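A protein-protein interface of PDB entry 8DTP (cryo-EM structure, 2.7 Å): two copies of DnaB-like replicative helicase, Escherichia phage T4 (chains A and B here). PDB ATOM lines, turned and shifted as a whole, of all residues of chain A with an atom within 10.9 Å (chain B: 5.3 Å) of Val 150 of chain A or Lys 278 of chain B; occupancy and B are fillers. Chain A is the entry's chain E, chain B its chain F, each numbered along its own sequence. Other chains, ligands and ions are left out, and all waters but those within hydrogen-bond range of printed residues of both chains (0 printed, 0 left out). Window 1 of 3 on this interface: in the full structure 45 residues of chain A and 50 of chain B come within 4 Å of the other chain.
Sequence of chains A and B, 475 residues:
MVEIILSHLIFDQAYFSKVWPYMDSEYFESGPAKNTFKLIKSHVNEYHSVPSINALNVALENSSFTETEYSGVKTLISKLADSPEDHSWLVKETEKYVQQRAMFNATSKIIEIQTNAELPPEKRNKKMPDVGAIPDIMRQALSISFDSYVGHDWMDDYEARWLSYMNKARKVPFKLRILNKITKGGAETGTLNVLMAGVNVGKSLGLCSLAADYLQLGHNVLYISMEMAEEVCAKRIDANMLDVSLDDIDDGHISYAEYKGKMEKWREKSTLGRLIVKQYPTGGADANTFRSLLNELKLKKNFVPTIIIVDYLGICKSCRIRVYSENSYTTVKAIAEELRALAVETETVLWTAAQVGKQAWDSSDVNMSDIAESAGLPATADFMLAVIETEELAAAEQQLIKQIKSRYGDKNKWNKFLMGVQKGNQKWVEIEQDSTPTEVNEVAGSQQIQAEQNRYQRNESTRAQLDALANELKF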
ATOM      1  N   LYS A  18     -21.568   9.511  35.235  1.00  0.00           N
ATOM      2  CA  LYS A  18     -21.553   9.331  33.791  1.00  0.00           C
ATOM      3  C   LYS A  18     -22.856   9.707  33.101  1.00  0.00           C
ATOM      4  O   LYS A  18     -22.845   9.913  31.883  1.00  0.00           O
ATOM      5  CB  LYS A  18     -21.210   7.876  33.435  1.00  0.00           C
ATOM      6  CG  LYS A  18     -20.616   7.704  32.047  1.00  0.00           C
ATOM      7  CD  LYS A  18     -20.292   6.251  31.751  1.00  0.00           C
ATOM      8  CE  LYS A  18     -19.557   6.115  30.426  1.00  0.00           C
ATOM      9  NZ  LYS A  18     -20.320   6.712  29.298  1.00  0.00           N
ATOM     10  N   TYR A  22     -25.729  14.433  31.310  1.00  0.00           N
ATOM     11  CA  TYR A  22     -26.753  14.443  30.236  1.00  0.00           C
ATOM     12  C   TYR A  22     -28.097  13.997  30.803  1.00  0.00           C
ATOM     13  O   TYR A  22     -28.436  12.813  30.649  1.00  0.00           O
ATOM     14  CB  TYR A  22     -26.345  13.470  29.133  1.00  0.00           C
ATOM     15  CG  TYR A  22     -24.863  13.230  29.014  1.00  0.00           C
ATOM     16  CD1 TYR A  22     -23.995  14.254  28.674  1.00  0.00           C
ATOM     17  CD2 TYR A  22     -24.324  11.977  29.252  1.00  0.00           C
ATOM     18  CE1 TYR A  22     -22.633  14.037  28.564  1.00  0.00           C
ATOM     19  CE2 TYR A  22     -22.965  11.743  29.145  1.00  0.00           C
ATOM     20  CZ  TYR A  22     -22.116  12.776  28.800  1.00  0.00           C
ATOM     21  OH  TYR A  22     -20.775  12.551  28.696  1.00  0.00           O
ATOM     22  N   SER A 145     -25.886  11.145  22.570  1.00  0.00           N
ATOM     23  CA  SER A 145     -25.202   9.963  23.071  1.00  0.00           C
ATOM     24  C   SER A 145     -24.416  10.292  24.336  1.00  0.00           C
ATOM     25  O   SER A 145     -24.008  11.434  24.564  1.00  0.00           O
ATOM     26  CB  SER A 145     -24.264   9.396  22.005  1.00  0.00           C
ATOM     27  OG  SER A 145     -23.263  10.335  21.656  1.00  0.00           O
ATOM     28  N   PHE A 146     -24.213   9.275  25.169  1.00  0.00           N
ATOM     29  CA  PHE A 146     -23.473   9.428  26.421  1.00  0.00           C
ATOM     30  C   PHE A 146     -21.997   9.187  26.138  1.00  0.00           C
ATOM     31  O   PHE A 146     -21.543   8.043  26.072  1.00  0.00           O
ATOM     32  CB  PHE A 146     -23.993   8.469  27.486  1.00  0.00           C
ATOM     33  CG  PHE A 146     -25.282   8.902  28.125  1.00  0.00           C
ATOM     34  CD1 PHE A 146     -26.041   9.921  27.576  1.00  0.00           C
ATOM     35  CD2 PHE A 146     -25.728   8.295  29.285  1.00  0.00           C
ATOM     36  CE1 PHE A 146     -27.223  10.317  28.167  1.00  0.00           C
ATOM     37  CE2 PHE A 146     -26.907   8.689  29.879  1.00  0.00           C
ATOM     38  CZ  PHE A 146     -27.654   9.702  29.321  1.00  0.00           C
ATOM     39  N   ASP A 147     -21.242  10.271  25.974  1.00  0.00           N
ATOM     40  CA  ASP A 147     -19.802  10.161  25.750  1.00  0.00           C
ATOM     41  C   ASP A 147     -19.165  11.477  26.175  1.00  0.00           C
ATOM     42  O   ASP A 147     -19.315  12.488  25.484  1.00  0.00           O
ATOM     43  CB  ASP A 147     -19.501   9.847  24.290  1.00  0.00           C
ATOM     44  CG  ASP A 147     -18.050   9.470  24.059  1.00  0.00           C
ATOM     45  OD1 ASP A 147     -17.298   9.349  25.048  1.00  0.00           O
ATOM     46  OD2 ASP A 147     -17.662   9.295  22.885  1.00  0.00           O
ATOM     47  N   SER A 148     -18.464  11.462  27.308  1.00  0.00           N
ATOM     48  CA  SER A 148     -17.780  12.643  27.814  1.00  0.00           C
ATOM     49  C   SER A 148     -16.327  12.729  27.369  1.00  0.00           C
ATOM     50  O   SER A 148     -15.711  13.788  27.524  1.00  0.00           O
ATOM     51  CB  SER A 148     -17.838  12.676  29.346  1.00  0.00           C
ATOM     52  OG  SER A 148     -17.205  11.538  29.904  1.00  0.00           O
ATOM     53  N   TYR A 149     -15.769  11.651  26.825  1.00  0.00           N
ATOM     54  CA  TYR A 149     -14.375  11.645  26.401  1.00  0.00           C
ATOM     55  C   TYR A 149     -14.260  12.299  25.030  1.00  0.00           C
ATOM     56  O   TYR A 149     -14.955  11.906  24.087  1.00  0.00           O
ATOM     57  CB  TYR A 149     -13.834  10.219  26.374  1.00  0.00           C
ATOM     58  CG  TYR A 149     -12.359  10.130  26.060  1.00  0.00           C
ATOM     59  CD1 TYR A 149     -11.419  10.735  26.882  1.00  0.00           C
ATOM     60  CD2 TYR A 149     -11.906   9.431  24.954  1.00  0.00           C
ATOM     61  CE1 TYR A 149     -10.070  10.655  26.603  1.00  0.00           C
ATOM     62  CE2 TYR A 149     -10.558   9.343  24.667  1.00  0.00           C
ATOM     63  CZ  TYR A 149      -9.645   9.958  25.495  1.00  0.00           C
ATOM     64  OH  TYR A 149      -8.301   9.874  25.213  1.00  0.00           O
ATOM     65  N   VAL A 150     -13.387  13.296  24.924  1.00  0.00           N
ATOM     66  CA  VAL A 150     -13.230  14.022  23.672  1.00  0.00           C
ATOM     67  C   VAL A 150     -12.069  13.488  22.839  1.00  0.00           C
ATOM     68  O   VAL A 150     -12.083  13.614  21.611  1.00  0.00           O
ATOM     69  CB  VAL A 150     -13.062  15.522  23.956  1.00  0.00           C
ATOM     70  CG1 VAL A 150     -14.342  16.093  24.547  1.00  0.00           C
ATOM     71  CG2 VAL A 150     -11.891  15.756  24.893  1.00  0.00           C
ATOM     72  N   GLY A 151     -11.064  12.900  23.472  1.00  0.00           N
ATOM     73  CA  GLY A 151      -9.949  12.292  22.775  1.00  0.00           C
ATOM     74  C   GLY A 151      -8.634  12.953  23.128  1.00  0.00           C
ATOM     75  O   GLY A 151      -8.548  13.817  24.006  1.00  0.00           O
ATOM     76  N   HIS A 152      -7.589  12.528  22.422  1.00  0.00           N
ATOM     77  CA  HIS A 152      -6.252  13.060  22.621  1.00  0.00           C
ATOM     78  C   HIS A 152      -6.199  14.535  22.223  1.00  0.00           C
ATOM     79  O   HIS A 152      -7.109  15.069  21.585  1.00  0.00           O
ATOM     80  CB  HIS A 152      -5.239  12.253  21.812  1.00  0.00           C
ATOM     81  CG  HIS A 152      -3.989  11.924  22.564  1.00  0.00           C
ATOM     82  ND1 HIS A 152      -4.002  11.296  23.791  1.00  0.00           N
ATOM     83  CD2 HIS A 152      -2.686  12.133  22.262  1.00  0.00           C
ATOM     84  CE1 HIS A 152      -2.762  11.134  24.212  1.00  0.00           C
ATOM     85  NE2 HIS A 152      -1.944  11.633  23.303  1.00  0.00           N
ATOM     86  N   ASP A 153      -5.115  15.199  22.614  1.00  0.00           N
ATOM     87  CA  ASP A 153      -4.919  16.605  22.282  1.00  0.00           C
ATOM     88  C   ASP A 153      -3.557  16.920  21.685  1.00  0.00           C
ATOM     89  O   ASP A 153      -3.397  18.012  21.123  1.00  0.00           O
ATOM     90  CB  ASP A 153      -5.126  17.485  23.523  1.00  0.00           C
ATOM     91  CG  ASP A 153      -5.484  18.913  23.169  1.00  0.00           C
ATOM     92  OD1 ASP A 153      -6.651  19.157  22.802  1.00  0.00           O
ATOM     93  OD2 ASP A 153      -4.602  19.791  23.253  1.00  0.00           O
ATOM     94  N   TRP A 154      -2.567  16.041  21.834  1.00  0.00           N
ATOM     95  CA  TRP A 154      -1.259  16.133  21.192  1.00  0.00           C
ATOM     96  C   TRP A 154      -0.392  17.233  21.798  1.00  0.00           C
ATOM     97  O   TRP A 154       0.814  17.287  21.542  1.00  0.00           O
ATOM     98  CB  TRP A 154      -1.414  16.352  19.680  1.00  0.00           C
ATOM     99  CG  TRP A 154      -0.113  16.384  18.950  1.00  0.00           C
ATOM    100  CD1 TRP A 154       0.563  15.321  18.440  1.00  0.00           C
ATOM    101  CD2 TRP A 154       0.679  17.542  18.660  1.00  0.00           C
ATOM    102  NE1 TRP A 154       1.729  15.740  17.848  1.00  0.00           N
ATOM    103  CE2 TRP A 154       1.824  17.101  17.973  1.00  0.00           C
ATOM    104  CE3 TRP A 154       0.534  18.907  18.920  1.00  0.00           C
ATOM    105  CZ2 TRP A 154       2.815  17.975  17.537  1.00  0.00           C
ATOM    106  CZ3 TRP A 154       1.517  19.772  18.488  1.00  0.00           C
ATOM    107  CH2 TRP A 154       2.643  19.304  17.804  1.00  0.00           C
ATOM    108  N   ASP A 156      -1.691  18.776  25.155  1.00  0.00           N
ATOM    109  CA  ASP A 156      -2.063  18.667  26.555  1.00  0.00           C
ATOM    110  C   ASP A 156      -1.873  17.263  27.108  1.00  0.00           C
ATOM    111  O   ASP A 156      -2.081  17.055  28.308  1.00  0.00           O
ATOM    112  CB  ASP A 156      -3.522  19.098  26.750  1.00  0.00           C
ATOM    113  CG  ASP A 156      -3.789  20.498  26.235  1.00  0.00           C
ATOM    114  OD1 ASP A 156      -2.841  21.145  25.743  1.00  0.00           O
ATOM    115  OD2 ASP A 156      -4.950  20.952  26.320  1.00  0.00           O
ATOM    116  N   ASP A 157      -1.475  16.302  26.272  1.00  0.00           N
ATOM    117  CA  ASP A 157      -1.377  14.906  26.677  1.00  0.00           C
ATOM    118  C   ASP A 157      -0.124  14.242  26.121  1.00  0.00           C
ATOM    119  O   ASP A 157      -0.101  13.023  25.926  1.00  0.00           O
ATOM    120  CB  ASP A 157      -2.618  14.128  26.238  1.00  0.00           C
ATOM    121  CG  ASP A 157      -3.892  14.660  26.862  1.00  0.00           C
ATOM    122  OD1 ASP A 157      -3.892  14.934  28.079  1.00  0.00           O
ATOM    123  OD2 ASP A 157      -4.894  14.806  26.134  1.00  0.00           O
ATOM    124  N   LEU B 222      -9.642  18.050  13.820  1.00  0.00           N
ATOM    125  CA  LEU B 222     -10.215  16.898  14.501  1.00  0.00           C
ATOM    126  C   LEU B 222      -9.951  15.664  13.651  1.00  0.00           C
ATOM    127  O   LEU B 222     -10.423  15.580  12.511  1.00  0.00           O
ATOM    128  CB  LEU B 222     -11.713  17.085  14.732  1.00  0.00           C
ATOM    129  CG  LEU B 222     -12.454  15.918  15.386  1.00  0.00           C
ATOM    130  CD1 LEU B 222     -11.972  15.700  16.810  1.00  0.00           C
ATOM    131  CD2 LEU B 222     -13.951  16.149  15.352  1.00  0.00           C
ATOM    132  N   TYR B 223      -9.204  14.715  14.201  1.00  0.00           N
ATOM    133  CA  TYR B 223      -8.852  13.481  13.510  1.00  0.00           C
ATOM    134  C   TYR B 223      -9.683  12.357  14.110  1.00  0.00           C
ATOM    135  O   TYR B 223      -9.408  11.899  15.224  1.00  0.00           O
ATOM    136  CB  TYR B 223      -7.358  13.190  13.629  1.00  0.00           C
ATOM    137  CG  TYR B 223      -6.868  12.087  12.718  1.00  0.00           C
ATOM    138  CD1 TYR B 223      -7.075  10.753  13.035  1.00  0.00           C
ATOM    139  CD2 TYR B 223      -6.188  12.379  11.547  1.00  0.00           C
ATOM    140  CE1 TYR B 223      -6.629   9.743  12.208  1.00  0.00           C
ATOM    141  CE2 TYR B 223      -5.735  11.375  10.714  1.00  0.00           C
ATOM    142  CZ  TYR B 223      -5.960  10.060  11.051  1.00  0.00           C
ATOM    143  OH  TYR B 223      -5.512   9.055  10.226  1.00  0.00           O
ATOM    144  N   ILE B 224     -10.697  11.917  13.375  1.00  0.00           N
ATOM    145  CA  ILE B 224     -11.535  10.804  13.797  1.00  0.00           C
ATOM    146  C   ILE B 224     -10.970   9.540  13.163  1.00  0.00           C
ATOM    147  O   ILE B 224     -11.122   9.312  11.960  1.00  0.00           O
ATOM    148  CB  ILE B 224     -13.001  11.023  13.410  1.00  0.00           C
ATOM    149  CG1 ILE B 224     -13.551  12.257  14.123  1.00  0.00           C
ATOM    150  CG2 ILE B 224     -13.826   9.796  13.749  1.00  0.00           C
ATOM    151  CD1 ILE B 224     -14.946  12.637  13.700  1.00  0.00           C
ATOM    152  N   SER B 225     -10.311   8.719  13.974  1.00  0.00           N
ATOM    153  CA  SER B 225      -9.699   7.482  13.513  1.00  0.00           C
ATOM    154  C   SER B 225     -10.639   6.328  13.822  1.00  0.00           C
ATOM    155  O   SER B 225     -11.015   6.119  14.979  1.00  0.00           O
ATOM    156  CB  SER B 225      -8.341   7.260  14.177  1.00  0.00           C
ATOM    157  OG  SER B 225      -8.474   7.133  15.582  1.00  0.00           O
ATOM    158  N   GLU B 230      -5.732   6.122  19.267  1.00  0.00           N
ATOM    159  CA  GLU B 230      -5.420   7.546  19.336  1.00  0.00           C
ATOM    160  C   GLU B 230      -3.919   7.775  19.439  1.00  0.00           C
ATOM    161  O   GLU B 230      -3.374   8.686  18.802  1.00  0.00           O
ATOM    162  CB  GLU B 230      -6.137   8.181  20.525  1.00  0.00           C
ATOM    163  CG  GLU B 230      -7.634   7.952  20.538  1.00  0.00           C
ATOM    164  CD  GLU B 230      -8.299   8.498  21.784  1.00  0.00           C
ATOM    165  OE1 GLU B 230      -7.581   9.016  22.665  1.00  0.00           O
ATOM    166  OE2 GLU B 230      -9.540   8.409  21.881  1.00  0.00           O
ATOM    167  N   ILE B 276      -7.075  17.291  17.843  1.00  0.00           N
ATOM    168  CA  ILE B 276      -7.726  16.380  18.777  1.00  0.00           C
ATOM    169  C   ILE B 276      -8.051  15.091  18.040  1.00  0.00           C
ATOM    170  O   ILE B 276      -8.751  15.113  17.021  1.00  0.00           O
ATOM    171  CB  ILE B 276      -8.987  17.003  19.393  1.00  0.00           C
ATOM    172  CG1 ILE B 276      -8.587  18.115  20.363  1.00  0.00           C
ATOM    173  CG2 ILE B 276      -9.828  15.947  20.085  1.00  0.00           C
ATOM    174  CD1 ILE B 276      -9.750  18.839  20.988  1.00  0.00           C
ATOM    175  N   VAL B 277      -7.543  13.973  18.552  1.00  0.00           N
ATOM    176  CA  VAL B 277      -7.706  12.664  17.931  1.00  0.00           C
ATOM    177  C   VAL B 277      -8.732  11.881  18.736  1.00  0.00           C
ATOM    178  O   VAL B 277      -8.564  11.682  19.945  1.00  0.00           O
ATOM    179  CB  VAL B 277      -6.373  11.905  17.851  1.00  0.00           C
ATOM    180  CG1 VAL B 277      -6.584  10.527  17.248  1.00  0.00           C
ATOM    181  CG2 VAL B 277      -5.361  12.698  17.042  1.00  0.00           C
ATOM    182  N   LYS B 278      -9.789  11.434  18.065  1.00  0.00           N
ATOM    183  CA  LYS B 278     -10.837  10.630  18.678  1.00  0.00           C
ATOM    184  C   LYS B 278     -10.933   9.300  17.947  1.00  0.00           C
ATOM    185  O   LYS B 278     -11.045   9.271  16.718  1.00  0.00           O
ATOM    186  CB  LYS B 278     -12.183  11.356  18.637  1.00  0.00           C
ATOM    187  CG  LYS B 278     -13.323  10.605  19.308  1.00  0.00           C
ATOM    188  CD  LYS B 278     -13.151  10.560  20.813  1.00  0.00           C
ATOM    189  CE  LYS B 278     -14.346   9.907  21.487  1.00  0.00           C
ATOM    190  NZ  LYS B 278     -14.526   8.497  21.052  1.00  0.00           N
ATOM    191  N   GLN B 279     -10.898   8.206  18.701  1.00  0.00           N
ATOM    192  CA  GLN B 279     -10.974   6.866  18.141  1.00  0.00           C
ATOM    193  C   GLN B 279     -12.351   6.270  18.391  1.00  0.00           C
ATOM    194  O   GLN B 279     -12.882   6.349  19.503  1.00  0.00           O
ATOM    195  CB  GLN B 279      -9.907   5.947  18.740  1.00  0.00           C
ATOM    196  CG  GLN B 279      -9.974   4.518  18.229  1.00  0.00           C
ATOM    197  CD  GLN B 279      -9.070   3.579  18.997  1.00  0.00           C
ATOM    198  OE1 GLN B 279      -8.492   3.951  20.019  1.00  0.00           O
ATOM    199  NE2 GLN B 279      -8.939   2.351  18.508  1.00  0.00           N
ATOM    200  N   TYR B 280     -12.922   5.676  17.349  1.00  0.00           N
ATOM    201  CA  TYR B 280     -14.179   4.957  17.449  1.00  0.00           C
ATOM    202  C   TYR B 280     -13.990   3.534  16.952  1.00  0.00           C
ATOM    203  O   TYR B 280     -13.159   3.283  16.072  1.00  0.00           O
ATOM    204  CB  TYR B 280     -15.284   5.639  16.631  1.00  0.00           C
ATOM    205  CG  TYR B 280     -15.772   6.955  17.188  1.00  0.00           C
ATOM    206  CD1 TYR B 280     -16.634   6.996  18.272  1.00  0.00           C
ATOM    207  CD2 TYR B 280     -15.394   8.157  16.612  1.00  0.00           C
ATOM    208  CE1 TYR B 280     -17.090   8.197  18.777  1.00  0.00           C
ATOM    209  CE2 TYR B 280     -15.846   9.360  17.109  1.00  0.00           C
ATOM    210  CZ  TYR B 280     -16.693   9.375  18.191  1.00  0.00           C
ATOM    211  OH  TYR B 280     -17.143  10.573  18.688  1.00  0.00           O
ATOM    212  N   LEU B 293     -19.904  14.559  19.191  1.00  0.00           N
ATOM    213  CA  LEU B 293     -18.514  14.843  19.534  1.00  0.00           C
ATOM    214  C   LEU B 293     -18.194  16.321  19.351  1.00  0.00           C
ATOM    215  O   LEU B 293     -17.503  16.920  20.181  1.00  0.00           O
ATOM    216  CB  LEU B 293     -17.583  13.981  18.684  1.00  0.00           C
ATOM    217  CG  LEU B 293     -16.082  14.234  18.826  1.00  0.00           C
ATOM    218  CD1 LEU B 293     -15.625  13.987  20.251  1.00  0.00           C
ATOM    219  CD2 LEU B 293     -15.300  13.370  17.851  1.00  0.00           C
ATOM    220  N   GLU B 296     -19.823  18.272  22.268  1.00  0.00           N
ATOM    221  CA  GLU B 296     -19.089  18.153  23.526  1.00  0.00           C
ATOM    222  C   GLU B 296     -17.731  18.843  23.452  1.00  0.00           C
ATOM    223  O   GLU B 296     -17.262  19.380  24.460  1.00  0.00           O
ATOM    224  CB  GLU B 296     -18.933  16.685  23.929  1.00  0.00           C
ATOM    225  CG  GLU B 296     -18.011  15.860  23.052  1.00  0.00           C
ATOM    226  CD  GLU B 296     -17.557  14.584  23.731  1.00  0.00           C
ATOM    227  OE1 GLU B 296     -17.457  14.578  24.976  1.00  0.00           O
ATOM    228  OE2 GLU B 296     -17.303  13.587  23.023  1.00  0.00           O
ATOM    229  N   LEU B 297     -17.091  18.847  22.279  1.00  0.00           N
ATOM    230  CA  LEU B 297     -15.835  19.573  22.122  1.00  0.00           C
ATOM    231  C   LEU B 297     -16.040  21.070  22.300  1.00  0.00           C
ATOM    232  O   LEU B 297     -15.229  21.744  22.944  1.00  0.00           O
ATOM    233  CB  LEU B 297     -15.226  19.281  20.752  1.00  0.00           C
ATOM    234  CG  LEU B 297     -14.441  17.980  20.612  1.00  0.00           C
ATOM    235  CD1 LEU B 297     -14.068  17.734  19.163  1.00  0.00           C
ATOM    236  CD2 LEU B 297     -13.205  18.049  21.474  1.00  0.00           C
ATOM    237  N   LYS B 300     -17.226  21.579  26.337  1.00  0.00           N
ATOM    238  CA  LYS B 300     -16.332  21.217  27.428  1.00  0.00           C
ATOM    239  C   LYS B 300     -14.876  21.584  27.177  1.00  0.00           C
ATOM    240  O   LYS B 300     -14.071  21.515  28.113  1.00  0.00           O
ATOM    241  CB  LYS B 300     -16.429  19.712  27.711  1.00  0.00           C
ATOM    242  CG  LYS B 300     -17.835  19.228  28.018  1.00  0.00           C
ATOM    243  CD  LYS B 300     -18.407  19.928  29.240  1.00  0.00           C
ATOM    244  CE  LYS B 300     -19.834  19.481  29.513  1.00  0.00           C
ATOM    245  NZ  LYS B 300     -19.923  18.012  29.739  1.00  0.00           N
ATOM    246  N   LYS B 301     -14.512  21.966  25.954  1.00  0.00           N
ATOM    247  CA  LYS B 301     -13.132  22.302  25.642  1.00  0.00           C
ATOM    248  C   LYS B 301     -12.993  23.580  24.825  1.00  0.00           C
ATOM    249  O   LYS B 301     -11.863  24.016  24.580  1.00  0.00           O
ATOM    250  CB  LYS B 301     -12.458  21.133  24.901  1.00  0.00           C
ATOM    251  CG  LYS B 301     -10.938  21.158  24.919  1.00  0.00           C
ATOM    252  CD  LYS B 301     -10.360  19.763  24.782  1.00  0.00           C
ATOM    253  CE  LYS B 301     -10.627  18.941  26.029  1.00  0.00           C
ATOM    254  NZ  LYS B 301     -10.025  19.564  27.240  1.00  0.00           N
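Printed residues of chain B within 4 Å of Asp 147 of chain A: Lys 278 and Glu 296. Printed residues of chain B within 4 Å of Ser 148 of chain A: Glu 296. Val 150 of chain A touches six residues of chain B. Asp 157 of chain A touches none of the printed residues of chain B. No residue of chain A comes within 4 Å of Ile 224 of chain B. No residue of chain A comes within 4 Å of Ser 225 of chain B. Printed residues of chain A within 4 Å of Glu 230 of chain B: Tyr 149 and His 152. Lys 278 of chain B touches just these residues of chain A: Asp 147, Tyr 149 and Val 150. No residue of chain A comes within 4 Å of Tyr 280 of chain B. Glu 296 of chain B touches just these residues of chain A: Asp 147, Ser 148, Tyr 149 and Val 150. Of chain A, only Val 150 (3.5 Å) comes within 4 Å of Leu 297 of chain B. The nearest residue of chain B that does not touch Val 150 of chain A is Val 277 of chain B (4.3 Å). The nearest residue of chain A that does not touch Lys 278 of chain B is Gly 151 of chain A (4.1 Å).
O of Tyr 149 of chain A touches CE of Lys 278 of chain B, 3.3 Å away. Val 150 of chain A touches Ile 276 of chain B (O to CG2, 3.6 Å). Val 150 of chain A touches Lys 278 of chain B. Glu 296 of chain B touches Val 150 of chain A. CD2 of Leu 297 of chain B touches CB of Val 150 of chain A, 3.5 Å away. Val 150 of chain A touches Lys 301 of chain B (CG2 to CE, 3.6 Å). Gly 151 of chain A touches Val 277 of chain B (CA to O, 3.2 Å). His 152 of chain A touches Glu 230 of chain B (N to OE1, 3.5 Å). His 152 of chain A touches Ile 276 of chain B (O to CA, 3.2 Å). CG1 of Ile 276 of chain B touches OD1 of Asp 153 of chain A (3.3 Å).
Of the 15 printed residues of chain B, 8 touch a printed residue of chain A. Printed residues of chain B that touch a printed residue of chain A: Glu 230, Ile 276, Val 277, Lys 278, Leu 293, Glu 296, Leu 297 and Lys 301. Hydrophobic or aromatic side chains of chain B within 4 Å of the printed part of chain A: Ile 276, Leu 293 and Leu 297. Hydrophobic or aromatic side chains of chain A that line the printed part of chain B: Tyr 149, Val 150 and His 152. Among the printed residues, 17 pairs touch across the chains. Among the printed residues, Asp or Glu carboxylates within 4 Å of a Lys or Arg side-chain nitrogen of the other chain: Asp 147 of chain A with Lys 278 of chain B (3.7 Å).
The side-chain carboxylate (OD1) of Asp 147 of chain A lies within hydrogen-bond range of the backbone NH (N) of Tyr 149 of chain A, at 3.3 Å. O of Tyr 223 of chain B sits at hydrogen-bond distance from N of Lys 278 of chain B, at 2.9 Å. OE2 of Glu 230 of chain B lies within hydrogen-bond range of N of Gln 279 of chain B, at 3.5 Å. O of Lys 278 of chain B lies within hydrogen-bond range of N of Ser 225 of chain B (2.9 Å). The backbone carbonyl oxygen (O) of Asp 157 of chain A is in hydrogen-bond range of a ring nitrogen (NE2) of His 152 of chain A, 3.5 Å away. The side-chain hydroxyl (OH) of Tyr 22 of chain A lies within hydrogen-bond range of the backbone NH (N) of Ser 148 of chain A (2.9 Å).
No position is printed for both chains. Of the 17 pairs that touch across the chains among the printed residues, none has its exchanged pair printed and touching as well.
OH of Tyr 149 of chain A lies within hydrogen-bond range of OE1 of Glu 230 of chain B (2.8 Å). The side-chain carboxylate of Glu 296 of chain B lies close to the backbone carbonyl oxygen of Tyr 149 of chain A. The backbone NH (N) of His 152 of chain A lies within hydrogen-bond range of the backbone carbonyl oxygen (O) of Val 277 of chain B (2.8 Å). The backbone carbonyl oxygen (O) of Ser 148 of chain A lies close to the side-chain carboxylate (OE1) of Glu 296 of chain B (3.2 Å). The backbone carbonyl oxygen of Asp 147 of chain A sits close to the side-chain carboxylate of Glu 296 of chain B, 2.8 Å away. The side-chain carboxylate (OD2) of Asp 147 of chain A lies within salt-bridge range of the side-chain amino group (NZ) of Lys 278 of chain B, 3.7 Å away.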
